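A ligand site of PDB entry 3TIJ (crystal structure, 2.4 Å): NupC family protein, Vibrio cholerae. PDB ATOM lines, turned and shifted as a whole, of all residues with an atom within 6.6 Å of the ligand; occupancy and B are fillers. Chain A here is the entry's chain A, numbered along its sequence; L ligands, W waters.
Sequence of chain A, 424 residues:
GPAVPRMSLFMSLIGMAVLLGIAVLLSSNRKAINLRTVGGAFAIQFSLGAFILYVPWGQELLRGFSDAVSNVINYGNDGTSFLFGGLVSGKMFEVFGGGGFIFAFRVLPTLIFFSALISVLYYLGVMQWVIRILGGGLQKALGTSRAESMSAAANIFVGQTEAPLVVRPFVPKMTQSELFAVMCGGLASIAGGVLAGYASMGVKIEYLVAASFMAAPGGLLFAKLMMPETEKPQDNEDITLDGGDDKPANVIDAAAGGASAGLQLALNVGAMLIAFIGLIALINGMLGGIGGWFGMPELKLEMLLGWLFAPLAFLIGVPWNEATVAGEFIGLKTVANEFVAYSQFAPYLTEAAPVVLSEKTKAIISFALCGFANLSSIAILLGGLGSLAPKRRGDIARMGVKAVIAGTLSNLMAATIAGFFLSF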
ATOM      1  N   LEU A 111      24.068 -23.514  13.485  1.00  0.00           N
ATOM      2  CA  LEU A 111      23.279 -24.426  14.293  1.00  0.00           C
ATOM      3  C   LEU A 111      24.175 -25.217  15.235  1.00  0.00           C
ATOM      4  O   LEU A 111      23.801 -25.535  16.357  1.00  0.00           O
ATOM      5  CB  LEU A 111      22.470 -25.397  13.415  1.00  0.00           C
ATOM      6  CG  LEU A 111      21.546 -24.857  12.320  1.00  0.00           C
ATOM      7  CD1 LEU A 111      20.631 -25.976  11.797  1.00  0.00           C
ATOM      8  CD2 LEU A 111      20.709 -23.708  12.805  1.00  0.00           C
ATOM      9  N   VAL A 158      14.676 -22.989  23.254  1.00  0.00           N
ATOM     10  CA  VAL A 158      15.016 -24.289  22.674  1.00  0.00           C
ATOM     11  C   VAL A 158      13.845 -24.967  21.960  1.00  0.00           C
ATOM     12  O   VAL A 158      12.703 -24.556  22.105  1.00  0.00           O
ATOM     13  CB  VAL A 158      15.655 -25.276  23.719  1.00  0.00           C
ATOM     14  CG1 VAL A 158      16.800 -24.605  24.440  1.00  0.00           C
ATOM     15  CG2 VAL A 158      14.607 -25.775  24.715  1.00  0.00           C
ATOM     16  N   GLY A 159      14.161 -25.999  21.192  1.00  0.00           N
ATOM     17  CA  GLY A 159      13.196 -26.677  20.349  1.00  0.00           C
ATOM     18  C   GLY A 159      12.177 -27.515  21.094  1.00  0.00           C
ATOM     19  O   GLY A 159      12.327 -27.816  22.276  1.00  0.00           O
ATOM     20  N   GLN A 160      11.142 -27.914  20.358  1.00  0.00           N
ATOM     21  CA  GLN A 160       9.980 -28.617  20.902  1.00  0.00           C
ATOM     22  C   GLN A 160      10.299 -29.923  21.645  1.00  0.00           C
ATOM     23  O   GLN A 160       9.560 -30.317  22.547  1.00  0.00           O
ATOM     24  CB  GLN A 160       8.998 -28.897  19.760  1.00  0.00           C
ATOM     25  CG  GLN A 160       9.545 -29.797  18.683  1.00  0.00           C
ATOM     26  CD  GLN A 160       8.710 -29.775  17.419  1.00  0.00           C
ATOM     27  OE1 GLN A 160       7.494 -29.576  17.473  1.00  0.00           O
ATOM     28  NE2 GLN A 160       9.354 -29.980  16.270  1.00  0.00           N
ATOM     29  N   THR A 161      11.374 -30.606  21.249  1.00  0.00           N
ATOM     30  CA  THR A 161      11.729 -31.883  21.886  1.00  0.00           C
ATOM     31  C   THR A 161      12.701 -31.676  23.052  1.00  0.00           C
ATOM     32  O   THR A 161      12.895 -32.570  23.871  1.00  0.00           O
ATOM     33  CB  THR A 161      12.311 -32.913  20.879  1.00  0.00           C
ATOM     34  OG1 THR A 161      13.423 -32.341  20.172  1.00  0.00           O
ATOM     35  CG2 THR A 161      11.265 -33.352  19.862  1.00  0.00           C
ATOM     36  N   GLU A 162      13.301 -30.496  23.131  1.00  0.00           N
ATOM     37  CA  GLU A 162      14.275 -30.180  24.177  1.00  0.00           C
ATOM     38  C   GLU A 162      13.607 -29.509  25.377  1.00  0.00           C
ATOM     39  O   GLU A 162      13.990 -29.737  26.512  1.00  0.00           O
ATOM     40  CB  GLU A 162      15.387 -29.281  23.626  1.00  0.00           C
ATOM     41  CG  GLU A 162      16.356 -29.979  22.670  1.00  0.00           C
ATOM     42  CD  GLU A 162      15.828 -30.043  21.226  1.00  0.00           C
ATOM     43  OE1 GLU A 162      14.600 -30.004  21.009  1.00  0.00           O
ATOM     44  OE2 GLU A 162      16.668 -30.127  20.292  1.00  0.00           O
ATOM     45  N   ILE A 190      10.184 -21.653  17.972  1.00  0.00           N
ATOM     46  CA  ILE A 190      11.293 -22.244  17.259  1.00  0.00           C
ATOM     47  C   ILE A 190      12.378 -22.602  18.270  1.00  0.00           C
ATOM     48  O   ILE A 190      12.080 -23.135  19.346  1.00  0.00           O
ATOM     49  CB  ILE A 190      11.812 -21.329  16.134  1.00  0.00           C
ATOM     50  CG1 ILE A 190      12.212 -19.957  16.679  1.00  0.00           C
ATOM     51  CG2 ILE A 190      10.741 -21.156  15.070  1.00  0.00           C
ATOM     52  CD1 ILE A 190      13.049 -19.153  15.697  1.00  0.00           C
ATOM     53  N   ALA A 191      13.635 -22.319  17.934  1.00  0.00           N
ATOM     54  CA  ALA A 191      14.755 -22.666  18.815  1.00  0.00           C
ATOM     55  C   ALA A 191      15.947 -21.775  18.504  1.00  0.00           C
ATOM     56  O   ALA A 191      16.088 -21.290  17.372  1.00  0.00           O
ATOM     57  CB  ALA A 191      15.112 -24.140  18.673  1.00  0.00           C
ATOM     58  N   GLY A 193      19.128 -22.245  17.892  1.00  0.00           N
ATOM     59  CA  GLY A 193      19.962 -22.635  16.771  1.00  0.00           C
ATOM     60  C   GLY A 193      19.456 -22.170  15.415  1.00  0.00           C
ATOM     61  O   GLY A 193      20.191 -21.524  14.666  1.00  0.00           O
ATOM     62  N   VAL A 194      18.206 -22.480  15.102  1.00  0.00           N
ATOM     63  CA  VAL A 194      17.635 -22.092  13.814  1.00  0.00           C
ATOM     64  C   VAL A 194      17.325 -20.596  13.751  1.00  0.00           C
ATOM     65  O   VAL A 194      17.370 -20.011  12.670  1.00  0.00           O
ATOM     66  CB  VAL A 194      16.392 -22.934  13.428  1.00  0.00           C
ATOM     67  CG1 VAL A 194      16.789 -24.383  13.158  1.00  0.00           C
ATOM     68  CG2 VAL A 194      15.319 -22.851  14.508  1.00  0.00           C
ATOM     69  N   TYR A 198      18.081 -18.275  10.597  1.00  0.00           N
ATOM     70  CA  TYR A 198      17.196 -17.344   9.902  1.00  0.00           C
ATOM     71  C   TYR A 198      17.769 -15.941   9.871  1.00  0.00           C
ATOM     72  O   TYR A 198      17.664 -15.241   8.858  1.00  0.00           O
ATOM     73  CB  TYR A 198      15.813 -17.360  10.556  1.00  0.00           C
ATOM     74  CG  TYR A 198      15.200 -18.739  10.556  1.00  0.00           C
ATOM     75  CD1 TYR A 198      15.466 -19.612   9.510  1.00  0.00           C
ATOM     76  CD2 TYR A 198      14.391 -19.178  11.592  1.00  0.00           C
ATOM     77  CE1 TYR A 198      14.936 -20.889   9.497  1.00  0.00           C
ATOM     78  CE2 TYR A 198      13.848 -20.459  11.584  1.00  0.00           C
ATOM     79  CZ  TYR A 198      14.127 -21.297  10.534  1.00  0.00           C
ATOM     80  OH  TYR A 198      13.604 -22.567  10.502  1.00  0.00           O
ATOM     81  N   LEU A 265      21.774 -32.106  13.745  1.00  0.00           N
ATOM     82  CA  LEU A 265      20.697 -31.238  13.299  1.00  0.00           C
ATOM     83  C   LEU A 265      21.054 -30.548  11.980  1.00  0.00           C
ATOM     84  O   LEU A 265      20.230 -30.488  11.078  1.00  0.00           O
ATOM     85  CB  LEU A 265      20.362 -30.198  14.377  1.00  0.00           C
ATOM     86  CG  LEU A 265      19.305 -29.145  14.022  1.00  0.00           C
ATOM     87  CD1 LEU A 265      17.950 -29.800  13.693  1.00  0.00           C
ATOM     88  CD2 LEU A 265      19.170 -28.169  15.170  1.00  0.00           C
ATOM     89  N   VAL A 269      18.939 -30.878   8.467  1.00  0.00           N
ATOM     90  CA  VAL A 269      18.310 -29.711   7.860  1.00  0.00           C
ATOM     91  C   VAL A 269      18.827 -29.508   6.435  1.00  0.00           C
ATOM     92  O   VAL A 269      18.068 -29.170   5.529  1.00  0.00           O
ATOM     93  CB  VAL A 269      18.515 -28.431   8.717  1.00  0.00           C
ATOM     94  CG1 VAL A 269      18.275 -27.154   7.876  1.00  0.00           C
ATOM     95  CG2 VAL A 269      17.624 -28.480   9.977  1.00  0.00           C
ATOM     96  N   MET A 272      17.265 -32.205   4.124  1.00  0.00           N
ATOM     97  CA  MET A 272      15.863 -31.868   3.937  1.00  0.00           C
ATOM     98  C   MET A 272      15.689 -30.712   2.920  1.00  0.00           C
ATOM     99  O   MET A 272      14.774 -30.729   2.102  1.00  0.00           O
ATOM    100  CB  MET A 272      15.198 -31.527   5.274  1.00  0.00           C
ATOM    101  CG  MET A 272      13.771 -30.958   5.168  1.00  0.00           C
ATOM    102  SD  MET A 272      13.669 -29.201   4.713  1.00  0.00           S
ATOM    103  CE  MET A 272      14.406 -28.419   6.151  1.00  0.00           C
ATOM    104  N   ALA A 336       4.830 -27.465   4.351  1.00  0.00           N
ATOM    105  CA  ALA A 336       6.150 -28.079   4.435  1.00  0.00           C
ATOM    106  C   ALA A 336       6.799 -27.844   5.805  1.00  0.00           C
ATOM    107  O   ALA A 336       6.625 -28.643   6.708  1.00  0.00           O
ATOM    108  CB  ALA A 336       7.051 -27.586   3.322  1.00  0.00           C
ATOM    109  N   ASN A 337       7.547 -26.738   5.927  1.00  0.00           N
ATOM    110  CA  ASN A 337       8.047 -26.267   7.222  1.00  0.00           C
ATOM    111  C   ASN A 337       8.585 -24.824   7.132  1.00  0.00           C
ATOM    112  O   ASN A 337       8.733 -24.294   6.040  1.00  0.00           O
ATOM    113  CB  ASN A 337       9.101 -27.219   7.820  1.00  0.00           C
ATOM    114  CG  ASN A 337      10.336 -27.360   6.926  1.00  0.00           C
ATOM    115  OD1 ASN A 337      11.087 -26.413   6.722  1.00  0.00           O
ATOM    116  ND2 ASN A 337      10.558 -28.577   6.413  1.00  0.00           N
ATOM    117  N   GLU A 338       8.867 -24.190   8.260  1.00  0.00           N
ATOM    118  CA  GLU A 338       9.254 -22.781   8.247  1.00  0.00           C
ATOM    119  C   GLU A 338      10.624 -22.545   7.604  1.00  0.00           C
ATOM    120  O   GLU A 338      10.911 -21.454   7.103  1.00  0.00           O
ATOM    121  CB  GLU A 338       9.193 -22.164   9.645  1.00  0.00           C
ATOM    122  CG  GLU A 338      10.434 -22.368  10.502  1.00  0.00           C
ATOM    123  CD  GLU A 338      10.656 -23.838  10.917  1.00  0.00           C
ATOM    124  OE1 GLU A 338       9.740 -24.678  10.709  1.00  0.00           O
ATOM    125  OE2 GLU A 338      11.750 -24.131  11.450  1.00  0.00           O
ATOM    126  N   PHE A 339      11.458 -23.577   7.610  1.00  0.00           N
ATOM    127  CA  PHE A 339      12.793 -23.431   7.072  1.00  0.00           C
ATOM    128  C   PHE A 339      12.779 -23.299   5.539  1.00  0.00           C
ATOM    129  O   PHE A 339      13.466 -22.435   4.988  1.00  0.00           O
ATOM    130  CB  PHE A 339      13.657 -24.602   7.512  1.00  0.00           C
ATOM    131  CG  PHE A 339      15.064 -24.229   7.802  1.00  0.00           C
ATOM    132  CD1 PHE A 339      15.664 -24.577   8.988  1.00  0.00           C
ATOM    133  CD2 PHE A 339      15.808 -23.528   6.874  1.00  0.00           C
ATOM    134  CE1 PHE A 339      16.988 -24.224   9.234  1.00  0.00           C
ATOM    135  CE2 PHE A 339      17.134 -23.185   7.142  1.00  0.00           C
ATOM    136  CZ  PHE A 339      17.715 -23.534   8.316  1.00  0.00           C
ATOM    137  N   VAL A 340      12.013 -24.158   4.865  1.00  0.00           N
ATOM    138  CA  VAL A 340      11.835 -24.035   3.414  1.00  0.00           C
ATOM    139  C   VAL A 340      11.204 -22.681   3.082  1.00  0.00           C
ATOM    140  O   VAL A 340      11.597 -22.043   2.121  1.00  0.00           O
ATOM    141  CB  VAL A 340      10.973 -25.184   2.810  1.00  0.00           C
ATOM    142  CG1 VAL A 340      10.800 -25.006   1.325  1.00  0.00           C
ATOM    143  CG2 VAL A 340      11.623 -26.509   3.104  1.00  0.00           C
ATOM    144  N   GLY A 371       7.510 -20.367  13.584  1.00  0.00           N
ATOM    145  CA  GLY A 371       7.016 -21.464  14.389  1.00  0.00           C
ATOM    146  C   GLY A 371       7.288 -22.828  13.775  1.00  0.00           C
ATOM    147  O   GLY A 371       7.427 -22.938  12.559  1.00  0.00           O
ATOM    148  N   PHE A 372       7.384 -23.857  14.623  1.00  0.00           N
ATOM    149  CA  PHE A 372       7.579 -25.230  14.178  1.00  0.00           C
ATOM    150  C   PHE A 372       6.240 -25.911  13.831  1.00  0.00           C
ATOM    151  O   PHE A 372       6.185 -27.119  13.577  1.00  0.00           O
ATOM    152  CB  PHE A 372       8.310 -26.056  15.253  1.00  0.00           C
ATOM    153  CG  PHE A 372       9.791 -25.760  15.354  1.00  0.00           C
ATOM    154  CD1 PHE A 372      10.430 -24.938  14.447  1.00  0.00           C
ATOM    155  CD2 PHE A 372      10.549 -26.335  16.370  1.00  0.00           C
ATOM    156  CE1 PHE A 372      11.778 -24.681  14.550  1.00  0.00           C
ATOM    157  CE2 PHE A 372      11.887 -26.068  16.478  1.00  0.00           C
ATOM    158  CZ  PHE A 372      12.508 -25.240  15.567  1.00  0.00           C
ATOM    159  N   ALA A 373       5.164 -25.120  13.807  1.00  0.00           N
ATOM    160  CA  ALA A 373       3.829 -25.642  13.495  1.00  0.00           C
ATOM    161  C   ALA A 373       3.687 -26.129  12.049  1.00  0.00           C
ATOM    162  O   ALA A 373       3.537 -25.335  11.130  1.00  0.00           O
ATOM    163  CB  ALA A 373       2.745 -24.604  13.811  1.00  0.00           C
ATOM    164  N   ASN A 374       3.756 -27.447  11.882  1.00  0.00           N
ATOM    165  CA  ASN A 374       3.491 -28.131  10.611  1.00  0.00           C
ATOM    166  C   ASN A 374       3.235 -29.608  10.925  1.00  0.00           C
ATOM    167  O   ASN A 374       3.535 -30.060  12.032  1.00  0.00           O
ATOM    168  CB  ASN A 374       4.629 -27.950   9.593  1.00  0.00           C
ATOM    169  CG  ASN A 374       5.968 -28.497  10.093  1.00  0.00           C
ATOM    170  OD1 ASN A 374       6.205 -29.717  10.095  1.00  0.00           O
ATOM    171  ND2 ASN A 374       6.854 -27.603  10.506  1.00  0.00           N
ATOM    172  N   SER A 376       4.664 -32.323   9.916  1.00  0.00           N
ATOM    173  CA  SER A 376       5.863 -33.153  10.138  1.00  0.00           C
ATOM    174  C   SER A 376       6.421 -33.051  11.561  1.00  0.00           C
ATOM    175  O   SER A 376       7.098 -33.980  12.042  1.00  0.00           O
ATOM    176  CB  SER A 376       6.944 -32.839   9.102  1.00  0.00           C
ATOM    177  OG  SER A 376       6.597 -33.408   7.843  1.00  0.00           O
ATOM    178  N   SER A 377       6.145 -31.939  12.232  1.00  0.00           N
ATOM    179  CA  SER A 377       6.565 -31.789  13.621  1.00  0.00           C
ATOM    180  C   SER A 377       5.868 -32.789  14.553  1.00  0.00           C
ATOM    181  O   SER A 377       6.352 -33.018  15.669  1.00  0.00           O
ATOM    182  CB  SER A 377       6.345 -30.361  14.112  1.00  0.00           C
ATOM    183  OG  SER A 377       7.319 -29.485  13.561  1.00  0.00           O
ATOM    184  N   ILE A 378       4.767 -33.393  14.101  1.00  0.00           N
ATOM    185  CA  ILE A 378       4.108 -34.423  14.924  1.00  0.00           C
ATOM    186  C   ILE A 378       4.974 -35.668  15.071  1.00  0.00           C
ATOM    187  O   ILE A 378       5.122 -36.189  16.166  1.00  0.00           O
ATOM    188  CB  ILE A 378       2.720 -34.850  14.389  1.00  0.00           C
ATOM    189  CG1 ILE A 378       1.828 -33.637  14.125  1.00  0.00           C
ATOM    190  CG2 ILE A 378       2.044 -35.818  15.370  1.00  0.00           C
ATOM    191  CD1 ILE A 378       0.595 -33.953  13.290  1.00  0.00           C
ATOM    192  N   ILE A 380       8.045 -35.835  14.944  1.00  0.00           N
ATOM    193  CA  ILE A 380       9.199 -35.453  15.753  1.00  0.00           C
ATOM    194  C   ILE A 380       8.833 -35.404  17.231  1.00  0.00           C
ATOM    195  O   ILE A 380       9.589 -35.884  18.074  1.00  0.00           O
ATOM    196  CB  ILE A 380       9.807 -34.122  15.254  1.00  0.00           C
ATOM    197  CG1 ILE A 380      10.515 -34.365  13.924  1.00  0.00           C
ATOM    198  CG2 ILE A 380      10.771 -33.532  16.292  1.00  0.00           C
ATOM    199  CD1 ILE A 380      11.048 -33.111  13.272  1.00  0.00           C
HETATM  200  N1  LIG L   1      13.167 -28.889  14.107  1.00  0.00           N
HETATM  201  C1  LIG L   1      13.018 -29.374  15.398  1.00  0.00           C
HETATM  202  N2  LIG L   1      13.905 -28.890  16.332  1.00  0.00           N
HETATM  203  C2  LIG L   1      14.914 -27.971  16.098  1.00  0.00           C
HETATM  204  C3  LIG L   1      15.013 -27.509  14.750  1.00  0.00           C
HETATM  205  C4  LIG L   1      14.167 -27.969  13.820  1.00  0.00           C
HETATM  206  O1  LIG L   1      12.151 -30.182  15.700  1.00  0.00           O
HETATM  207  O2  LIG L   1      15.625 -27.634  17.049  1.00  0.00           O
HETATM  208  C5  LIG L   1      12.230 -29.422  13.085  1.00  0.00           C
HETATM  209  C6  LIG L   1      10.837 -28.774  13.173  1.00  0.00           C
HETATM  210  C7  LIG L   1      10.959 -27.652  12.143  1.00  0.00           C
HETATM  211  C8  LIG L   1      11.837 -28.291  11.062  1.00  0.00           C
HETATM  212  O3  LIG L   1       9.867 -29.723  12.759  1.00  0.00           O
HETATM  213  O4  LIG L   1       9.717 -27.190  11.657  1.00  0.00           O
HETATM  214  O5  LIG L   1      12.750 -29.146  11.796  1.00  0.00           O
HETATM  215  C9  LIG L   1      12.615 -27.331  10.187  1.00  0.00           C
HETATM  216  O6  LIG L   1      13.231 -26.301  10.959  1.00  0.00           O
HETATM  217  O   HOH W   1       8.889 -30.432  10.101  1.00  0.00           O
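O6 of the ligand lies within hydrogen-bond range of OE2 of Glu 338, at 2.7 Å. The side-chain hydroxyl of Ser 377 lies within hydrogen-bond range of an oxygen (O3) of the ligand (2.7 Å). The side-chain amide nitrogen (NE2) of Gln 160 sits at hydrogen-bond distance from an oxygen (O1) of the ligand (2.9 Å). O4 of the ligand lies within hydrogen-bond range of ND2 of Asn 374 (3.1 Å).
NE2 of Gln 160 is in hydrogen-bond range of OG of Ser 377 (3.4 Å). The backbone carbonyl oxygen (O) of Phe 372 sits at hydrogen-bond distance from the side-chain amide nitrogen (ND2) of Asn 374 (3.2 Å). The side-chain amide nitrogen of Asn 337 sits at hydrogen-bond distance from the side-chain sulfur of Met 272 (3.6 Å). The side-chain amide oxygen (OD1) of Asn 337 sits at hydrogen-bond distance from the backbone NH (N) of Val 340 (3.1 Å). OE2 of Glu 338 sits at hydrogen-bond distance from OH of Tyr 198 (2.6 Å). The backbone NH (N) of Phe 339 lies within hydrogen-bond range of the side-chain amide oxygen (OD1) of Asn 337, at 3.0 Å. OG of Ser 377 lies within hydrogen-bond range of O of Phe 372. The backbone NH (N) of Ser 377 is in hydrogen-bond range of the side-chain amide oxygen (OD1) of Asn 374 (3.1 Å).
CB of Ala 191 touches O2 of the ligand, 3.9 Å away. Val 194 touches the ligand. Tyr 198 touches the ligand. Leu 265 touches the ligand. CB of Asn 337 touches O4 of the ligand, 3.9 Å away. Phe 339 touches the ligand (CD1 to O6, 3.6 Å). Phe 372 touches the ligand. CD1 of Ile 380 touches O3 of the ligand (3.6 Å). Hydrophobic or aromatic side chains that line the ligand: Ala 191, Val 194, Leu 265, Phe 339, Phe 372 and Ile 380. Along chain A the residues within 4 Å of the ligand span positions 160 to 380.
Water W1 lies within hydrogen-bond range of the side-chain amide oxygen (OD1) of Asn 374 (2.8 Å) and an oxygen (O3) of the ligand (2.9 Å).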
